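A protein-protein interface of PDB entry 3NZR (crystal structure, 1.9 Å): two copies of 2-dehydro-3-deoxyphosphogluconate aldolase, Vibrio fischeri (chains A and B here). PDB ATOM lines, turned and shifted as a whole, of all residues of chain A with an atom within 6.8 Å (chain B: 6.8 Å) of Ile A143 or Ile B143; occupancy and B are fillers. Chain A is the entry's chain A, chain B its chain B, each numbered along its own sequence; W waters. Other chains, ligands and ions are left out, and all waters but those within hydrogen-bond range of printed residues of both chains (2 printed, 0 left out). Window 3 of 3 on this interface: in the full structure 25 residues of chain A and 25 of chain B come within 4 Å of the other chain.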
ATOM      1  N   THR A 122       4.904   2.847   4.265  1.00  0.00           N
ATOM      2  CA  THR A 122       5.367   4.212   4.404  1.00  0.00           C
ATOM      3  C   THR A 122       5.808   4.874   3.094  1.00  0.00           C
ATOM      4  O   THR A 122       6.119   6.046   3.091  1.00  0.00           O
ATOM      5  CB  THR A 122       6.595   4.259   5.314  1.00  0.00           C
ATOM      6  OG1 THR A 122       7.652   3.506   4.692  1.00  0.00           O
ATOM      7  CG2 THR A 122       6.248   3.760   6.733  1.00  0.00           C
ATOM      8  N   THR A 124       8.499   3.687   1.700  1.00  0.00           N
ATOM      9  CA  THR A 124       9.921   3.392   1.701  1.00  0.00           C
ATOM     10  C   THR A 124      10.007   1.908   1.999  1.00  0.00           C
ATOM     11  O   THR A 124       9.573   1.481   3.067  1.00  0.00           O
ATOM     12  CB  THR A 124      10.670   4.209   2.797  1.00  0.00           C
ATOM     13  OG1 THR A 124      10.501   5.603   2.531  1.00  0.00           O
ATOM     14  CG2 THR A 124      12.113   3.889   2.842  1.00  0.00           C
ATOM     15  N   MET A 127      10.868   0.185   5.621  1.00  0.00           N
ATOM     16  CA  MET A 127      10.455   0.968   6.743  1.00  0.00           C
ATOM     17  C   MET A 127       8.949   0.873   6.943  1.00  0.00           C
ATOM     18  O   MET A 127       8.165   0.899   5.957  1.00  0.00           O
ATOM     19  CB  MET A 127      10.823   2.440   6.560  1.00  0.00           C
ATOM     20  CG  MET A 127      12.305   2.697   6.321  1.00  0.00           C
ATOM     21  SD  MET A 127      13.414   2.274   7.907  1.00  0.00           S
ATOM     22  CE  MET A 127      13.004   3.771   9.153  1.00  0.00           C
ATOM     23  N   VAL A 128       8.544   0.783   8.211  1.00  0.00           N
ATOM     24  CA  VAL A 128       7.122   0.609   8.526  1.00  0.00           C
ATOM     25  C   VAL A 128       6.665   1.534   9.630  1.00  0.00           C
ATOM     26  O   VAL A 128       7.457   1.892  10.520  1.00  0.00           O
ATOM     27  CB  VAL A 128       6.753  -0.847   8.925  1.00  0.00           C
ATOM     28  CG1 VAL A 128       6.945  -1.854   7.750  1.00  0.00           C
ATOM     29  CG2 VAL A 128       7.489  -1.263  10.192  1.00  0.00           C
ATOM     30  N   LYS A 129       5.390   1.916   9.568  1.00  0.00           N
ATOM     31  CA  LYS A 129       4.777   2.825  10.549  1.00  0.00           C
ATOM     32  C   LYS A 129       4.158   1.978  11.693  1.00  0.00           C
ATOM     33  O   LYS A 129       3.354   1.084  11.421  1.00  0.00           O
ATOM     34  CB  LYS A 129       3.747   3.763   9.955  1.00  0.00           C
ATOM     35  CG  LYS A 129       2.915   4.557  10.952  1.00  0.00           C
ATOM     36  CD  LYS A 129       1.793   5.377  10.332  1.00  0.00           C
ATOM     37  CE  LYS A 129       0.778   5.943  11.431  1.00  0.00           C
ATOM     38  NZ  LYS A 129      -0.161   6.903  10.794  1.00  0.00           N
ATOM     39  N   ILE A 130       4.524   2.270  12.931  1.00  0.00           N
ATOM     40  CA  ILE A 130       4.036   1.446  14.066  1.00  0.00           C
ATOM     41  C   ILE A 130       3.211   2.252  15.083  1.00  0.00           C
ATOM     42  O   ILE A 130       2.751   1.688  16.159  1.00  0.00           O
ATOM     43  CB  ILE A 130       5.188   0.748  14.818  1.00  0.00           C
ATOM     44  CG1 ILE A 130       6.203   1.771  15.323  1.00  0.00           C
ATOM     45  CG2 ILE A 130       5.924  -0.274  13.885  1.00  0.00           C
ATOM     46  CD1 ILE A 130       7.229   1.205  16.274  1.00  0.00           C
ATOM     47  N   SER A 131       3.057   3.556  14.854  1.00  0.00           N
ATOM     48  CA  SER A 131       2.297   4.395  15.783  1.00  0.00           C
ATOM     49  C   SER A 131       0.793   4.309  15.409  1.00  0.00           C
ATOM     50  O   SER A 131       0.174   5.334  14.987  1.00  0.00           O
ATOM     51  CB  SER A 131       2.774   5.850  15.709  1.00  0.00           C
ATOM     52  OG  SER A 131       3.073   6.229  14.365  1.00  0.00           O
ATOM     53  N   GLU A 140       3.029  12.433  15.402  1.00  0.00           N
ATOM     54  CA  GLU A 140       3.988  12.296  14.284  1.00  0.00           C
ATOM     55  C   GLU A 140       4.338  10.826  14.062  1.00  0.00           C
ATOM     56  O   GLU A 140       4.492  10.079  15.046  1.00  0.00           O
ATOM     57  CB  GLU A 140       5.255  13.102  14.625  1.00  0.00           C
ATOM     58  CG  GLU A 140       6.323  13.074  13.537  1.00  0.00           C
ATOM     59  CD  GLU A 140       7.520  14.015  13.806  1.00  0.00           C
ATOM     60  OE1 GLU A 140       7.553  14.685  14.899  1.00  0.00           O
ATOM     61  OE2 GLU A 140       8.437  14.037  12.921  1.00  0.00           O
ATOM     62  N   ASP A 141       4.444  10.375  12.810  1.00  0.00           N
ATOM     63  CA  ASP A 141       4.581   8.930  12.567  1.00  0.00           C
ATOM     64  C   ASP A 141       5.871   8.384  13.236  1.00  0.00           C
ATOM     65  O   ASP A 141       6.934   9.055  13.232  1.00  0.00           O
ATOM     66  CB  ASP A 141       4.544   8.598  11.050  1.00  0.00           C
ATOM     67  CG  ASP A 141       3.153   8.931  10.382  1.00  0.00           C
ATOM     68  OD1 ASP A 141       2.170   9.190  11.118  1.00  0.00           O
ATOM     69  OD2 ASP A 141       3.042   8.951   9.134  1.00  0.00           O
ATOM     70  N   ALA A 142       5.789   7.179  13.800  1.00  0.00           N
ATOM     71  CA  ALA A 142       6.947   6.426  14.229  1.00  0.00           C
ATOM     72  C   ALA A 142       7.241   5.443  13.139  1.00  0.00           C
ATOM     73  O   ALA A 142       6.457   4.518  12.922  1.00  0.00           O
ATOM     74  CB  ALA A 142       6.642   5.706  15.533  1.00  0.00           C
ATOM     75  N   ILE A 143       8.347   5.633  12.439  1.00  0.00           N
ATOM     76  CA  ILE A 143       8.673   4.824  11.256  1.00  0.00           C
ATOM     77  C   ILE A 143       9.959   4.097  11.569  1.00  0.00           C
ATOM     78  O   ILE A 143      10.977   4.724  11.960  1.00  0.00           O
ATOM     79  CB  ILE A 143       8.834   5.735   9.964  1.00  0.00           C
ATOM     80  CG1 ILE A 143       7.456   6.289   9.570  1.00  0.00           C
ATOM     81  CG2 ILE A 143       9.437   4.962   8.757  1.00  0.00           C
ATOM     82  CD1 ILE A 143       7.451   7.585   8.836  1.00  0.00           C
ATOM     83  N   VAL A 144       9.936   2.785  11.455  1.00  0.00           N
ATOM     84  CA  VAL A 144      11.040   1.998  11.937  1.00  0.00           C
ATOM     85  C   VAL A 144      11.365   0.862  10.989  1.00  0.00           C
ATOM     86  O   VAL A 144      10.565   0.491  10.097  1.00  0.00           O
ATOM     87  CB  VAL A 144      10.679   1.382  13.319  1.00  0.00           C
ATOM     88  CG1 VAL A 144      10.248   2.447  14.262  1.00  0.00           C
ATOM     89  CG2 VAL A 144       9.577   0.321  13.118  1.00  0.00           C
ATOM     90  N   PRO A 145      12.526   0.255  11.196  1.00  0.00           N
ATOM     91  CA  PRO A 145      12.902  -0.816  10.308  1.00  0.00           C
ATOM     92  C   PRO A 145      11.950  -2.014  10.479  1.00  0.00           C
ATOM     93  O   PRO A 145      11.581  -2.343  11.627  1.00  0.00           O
ATOM     94  CB  PRO A 145      14.313  -1.174  10.801  1.00  0.00           C
ATOM     95  CG  PRO A 145      14.812  -0.014  11.400  1.00  0.00           C
ATOM     96  CD  PRO A 145      13.643   0.616  12.103  1.00  0.00           C
ATOM     97  N   SER B 120      15.611   5.605  25.198  1.00  0.00           N
ATOM     98  CA  SER B 120      17.004   5.953  25.245  1.00  0.00           C
ATOM     99  C   SER B 120      17.384   7.125  24.310  1.00  0.00           C
ATOM    100  O   SER B 120      16.755   7.308  23.287  1.00  0.00           O
ATOM    101  CB  SER B 120      17.790   4.713  24.845  1.00  0.00           C
ATOM    102  OG  SER B 120      17.598   3.663  25.845  1.00  0.00           O
ATOM    103  N   PRO B 121      18.410   7.917  24.690  1.00  0.00           N
ATOM    104  CA  PRO B 121      18.923   8.970  23.834  1.00  0.00           C
ATOM    105  C   PRO B 121      19.505   8.379  22.545  1.00  0.00           C
ATOM    106  O   PRO B 121      19.819   7.195  22.463  1.00  0.00           O
ATOM    107  CB  PRO B 121      20.029   9.645  24.668  1.00  0.00           C
ATOM    108  CG  PRO B 121      20.194   8.897  25.917  1.00  0.00           C
ATOM    109  CD  PRO B 121      19.060   7.868  26.006  1.00  0.00           C
ATOM    110  N   THR B 122      19.585   9.214  21.523  1.00  0.00           N
ATOM    111  CA  THR B 122      20.033   8.811  20.208  1.00  0.00           C
ATOM    112  C   THR B 122      21.135   9.738  19.675  1.00  0.00           C
ATOM    113  O   THR B 122      21.619   9.501  18.605  1.00  0.00           O
ATOM    114  CB  THR B 122      18.913   8.937  19.163  1.00  0.00           C
ATOM    115  OG1 THR B 122      18.469  10.284  19.178  1.00  0.00           O
ATOM    116  CG2 THR B 122      17.709   7.954  19.423  1.00  0.00           C
ATOM    117  N   THR B 124      20.250  12.773  18.831  1.00  0.00           N
ATOM    118  CA  THR B 124      19.427  13.805  18.122  1.00  0.00           C
ATOM    119  C   THR B 124      18.297  14.349  19.011  1.00  0.00           C
ATOM    120  O   THR B 124      17.433  13.583  19.458  1.00  0.00           O
ATOM    121  CB  THR B 124      18.876  13.235  16.812  1.00  0.00           C
ATOM    122  OG1 THR B 124      19.980  12.983  15.943  1.00  0.00           O
ATOM    123  CG2 THR B 124      17.901  14.207  16.121  1.00  0.00           C
ATOM    124  N   MET B 127      14.430  12.923  19.277  1.00  0.00           N
ATOM    125  CA  MET B 127      14.285  11.572  18.794  1.00  0.00           C
ATOM    126  C   MET B 127      14.765  10.600  19.864  1.00  0.00           C
ATOM    127  O   MET B 127      15.777  10.855  20.548  1.00  0.00           O
ATOM    128  CB  MET B 127      15.107  11.380  17.549  1.00  0.00           C
ATOM    129  CG  MET B 127      14.740  12.361  16.434  1.00  0.00           C
ATOM    130  SD  MET B 127      12.892  12.029  15.704  1.00  0.00           S
ATOM    131  CE  MET B 127      13.049  10.341  14.768  1.00  0.00           C
ATOM    132  N   VAL B 128      14.021   9.522  20.067  1.00  0.00           N
ATOM    133  CA  VAL B 128      14.389   8.542  21.139  1.00  0.00           C
ATOM    134  C   VAL B 128      14.347   7.159  20.598  1.00  0.00           C
ATOM    135  O   VAL B 128      13.642   6.871  19.637  1.00  0.00           O
ATOM    136  CB  VAL B 128      13.470   8.623  22.347  1.00  0.00           C
ATOM    137  CG1 VAL B 128      13.675   9.992  23.101  1.00  0.00           C
ATOM    138  CG2 VAL B 128      11.969   8.360  21.935  1.00  0.00           C
ATOM    139  N   LYS B 129      15.128   6.278  21.213  1.00  0.00           N
ATOM    140  CA  LYS B 129      15.179   4.903  20.813  1.00  0.00           C
ATOM    141  C   LYS B 129      14.232   4.103  21.708  1.00  0.00           C
ATOM    142  O   LYS B 129      14.310   4.178  22.944  1.00  0.00           O
ATOM    143  CB  LYS B 129      16.593   4.383  20.903  1.00  0.00           C
ATOM    144  CG  LYS B 129      16.815   2.889  20.771  1.00  0.00           C
ATOM    145  CD  LYS B 129      18.130   2.382  21.364  1.00  0.00           C
ATOM    146  CE  LYS B 129      18.243   0.863  20.971  1.00  0.00           C
ATOM    147  NZ  LYS B 129      18.814  -0.185  21.948  1.00  0.00           N
ATOM    148  N   ILE B 130      13.354   3.329  21.053  1.00  0.00           N
ATOM    149  CA  ILE B 130      12.298   2.595  21.752  1.00  0.00           C
ATOM    150  C   ILE B 130      12.427   1.063  21.608  1.00  0.00           C
ATOM    151  O   ILE B 130      11.659   0.311  22.209  1.00  0.00           O
ATOM    152  CB  ILE B 130      10.872   2.988  21.280  1.00  0.00           C
ATOM    153  CG1 ILE B 130      10.651   2.660  19.842  1.00  0.00           C
ATOM    154  CG2 ILE B 130      10.498   4.431  21.611  1.00  0.00           C
ATOM    155  CD1 ILE B 130       9.207   2.863  19.494  1.00  0.00           C
ATOM    156  N   SER B 131      13.373   0.587  20.794  1.00  0.00           N
ATOM    157  CA  SER B 131      13.614  -0.816  20.661  1.00  0.00           C
ATOM    158  C   SER B 131      14.460  -1.381  21.838  1.00  0.00           C
ATOM    159  O   SER B 131      15.564  -1.800  21.616  1.00  0.00           O
ATOM    160  CB  SER B 131      14.355  -1.067  19.339  1.00  0.00           C
ATOM    161  OG  SER B 131      15.323  -0.035  19.116  1.00  0.00           O
ATOM    162  N   GLU B 140      18.369  -3.548  14.561  1.00  0.00           N
ATOM    163  CA  GLU B 140      18.518  -2.169  14.121  1.00  0.00           C
ATOM    164  C   GLU B 140      17.614  -1.205  14.955  1.00  0.00           C
ATOM    165  O   GLU B 140      16.415  -1.450  15.162  1.00  0.00           O
ATOM    166  CB  GLU B 140      18.244  -2.053  12.597  1.00  0.00           C
ATOM    167  CG  GLU B 140      18.491  -0.658  12.026  1.00  0.00           C
ATOM    168  CD  GLU B 140      18.285  -0.536  10.486  1.00  0.00           C
ATOM    169  OE1 GLU B 140      18.075  -1.571   9.784  1.00  0.00           O
ATOM    170  OE2 GLU B 140      18.341   0.624   9.995  1.00  0.00           O
ATOM    171  N   ASP B 141      18.198  -0.100  15.412  1.00  0.00           N
ATOM    172  CA  ASP B 141      17.478   0.819  16.280  1.00  0.00           C
ATOM    173  C   ASP B 141      16.153   1.342  15.712  1.00  0.00           C
ATOM    174  O   ASP B 141      16.080   1.736  14.597  1.00  0.00           O
ATOM    175  CB  ASP B 141      18.343   2.011  16.683  1.00  0.00           C
ATOM    176  CG  ASP B 141      19.519   1.629  17.588  1.00  0.00           C
ATOM    177  OD1 ASP B 141      19.566   0.479  18.054  1.00  0.00           O
ATOM    178  OD2 ASP B 141      20.380   2.505  17.857  1.00  0.00           O
ATOM    179  N   ALA B 142      15.122   1.336  16.576  1.00  0.00           N
ATOM    180  CA  ALA B 142      13.859   1.960  16.335  1.00  0.00           C
ATOM    181  C   ALA B 142      13.922   3.358  16.905  1.00  0.00           C
ATOM    182  O   ALA B 142      13.855   3.527  18.116  1.00  0.00           O
ATOM    183  CB  ALA B 142      12.745   1.175  17.066  1.00  0.00           C
ATOM    184  N   ILE B 143      13.989   4.369  16.038  1.00  0.00           N
ATOM    185  CA  ILE B 143      14.180   5.740  16.512  1.00  0.00           C
ATOM    186  C   ILE B 143      12.993   6.566  16.132  1.00  0.00           C
ATOM    187  O   ILE B 143      12.684   6.659  14.986  1.00  0.00           O
ATOM    188  CB  ILE B 143      15.432   6.402  15.877  1.00  0.00           C
ATOM    189  CG1 ILE B 143      16.714   5.703  16.309  1.00  0.00           C
ATOM    190  CG2 ILE B 143      15.471   7.839  16.219  1.00  0.00           C
ATOM    191  CD1 ILE B 143      16.658   5.364  17.703  1.00  0.00           C
ATOM    192  N   VAL B 144      12.334   7.180  17.111  1.00  0.00           N
ATOM    193  CA  VAL B 144      11.050   7.850  16.875  1.00  0.00           C
ATOM    194  C   VAL B 144      10.977   9.152  17.618  1.00  0.00           C
ATOM    195  O   VAL B 144      11.775   9.382  18.595  1.00  0.00           O
ATOM    196  CB  VAL B 144       9.872   6.937  17.292  1.00  0.00           C
ATOM    197  CG1 VAL B 144      10.112   5.505  16.693  1.00  0.00           C
ATOM    198  CG2 VAL B 144       9.733   6.925  18.849  1.00  0.00           C
ATOM    199  N   PRO B 145      10.035  10.032  17.193  1.00  0.00           N
ATOM    200  CA  PRO B 145       9.805  11.320  17.879  1.00  0.00           C
ATOM    201  C   PRO B 145       9.396  11.092  19.296  1.00  0.00           C
ATOM    202  O   PRO B 145       8.583  10.198  19.604  1.00  0.00           O
ATOM    203  CB  PRO B 145       8.626  11.963  17.104  1.00  0.00           C
ATOM    204  CG  PRO B 145       8.644  11.233  15.767  1.00  0.00           C
ATOM    205  CD  PRO B 145       9.084   9.841  16.056  1.00  0.00           C
HETATM  206  O   HOH W   1      10.147   7.727  13.484  1.00  0.00           O
HETATM  207  O   HOH W   2      13.747   3.937  13.244  1.00  0.00           O
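O of Val A144 is in hydrogen-bond range of N of Val A128 (2.8 Å).
OD1 of Asp A141 lies within salt-bridge range of NZ of Lys A129 (3.3 Å).
The backbone carbonyl oxygen of Ala A142 lies within hydrogen-bond range of the backbone NH of Ile A130 (3.0 Å).
The backbone NH (N) of Val B128 is in hydrogen-bond range of the backbone carbonyl oxygen (O) of Val B144, at 2.7 Å.
The backbone NH (N) of Ile B130 sits at hydrogen-bond distance from the backbone carbonyl oxygen (O) of Ala B142, at 3.0 Å.
OG of Ser B131 lies within hydrogen-bond range of N of Ala B142, 2.9 Å away.
Among the printed residues, pairs that only touch across the chains: Glu A140 with Pro B145 (3.6 Å), Asp A141 with Pro B145 (3.6 Å), Ala A142 with Val B144 (3.7 Å), Ile A143 with Ile B143 (3.98 Å), Val A144 with Ala B142 (3.96 Å), Val A144 with Val B144 (3.9 Å), Pro A145 with Glu B140 (3.6 Å) and Pro A145 with Asp B141 (3.7 Å).
Of chain B, only Ile B143 comes within 4 Å of Ile A143.
Ile B143 touches just one residue of chain A: Ile A143 (3.98 Å).
Printed residues of chain B within 4 Å of Glu A140: Pro B145 (3.6 Å).
Of the printed residues of chain A, Ala B142 touches Val A144.
Of the printed residues of chain A, Pro B145 touches Glu A140 and Asp A141.
Printed residues of chain B within 4 Å of Ala A142: Val B144.
Thr A124 touches none of the printed residues of chain B.
Lys B129 touches none of the printed residues of chain A.
The nearest residue of chain B that does not touch Ile A143 is Val B144 (4.6 Å).
The nearest residue of chain A that does not touch Ile B143 is Val A144 (4.6 Å).
The nearest printed residue of chain A that does not touch Glu B140 is Met A127 (5.6 Å).
Of the 13 printed residues of chain A, 6 touch a printed residue of chain B.
Hydrophobic or aromatic side chains of chain A that line the printed part of chain B: Ala A142, Val A144 and Pro A145.
Hydrophobic or aromatic side chains of chain B that line the printed part of chain A: Ala B142, Val B144 and Pro B145.
Among the printed residues, 8 pairs touch across the chains.
Among the printed residues, no Asp or Glu carboxylate lies within 4 Å of a Lys or Arg side-chain nitrogen of the other chain.
Glu A140 touches Pro B145, and with the chains exchanged Pro A145 touches Glu B140.
Asp A141 touches Pro B145, and with the chains exchanged Pro A145 touches Asp B141.
Ala A142 touches Val B144, and with the chains exchanged Val A144 touches Ala B142.
Ile A143 touches its own counterpart, Ile B143.
13 positions are printed for both chains.
Water W2 lies within hydrogen-bond range of the backbone NH (N) of Ile B143, the backbone carbonyl oxygen (O) of Ile A143 and the backbone carbonyl oxygen (O) of Asp B141.
Water W1 lies within hydrogen-bond range of N of Ile A143 (3.0 Å), O of Ile B143 (3.1 Å) and O of Asp A141 (3.5 Å).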
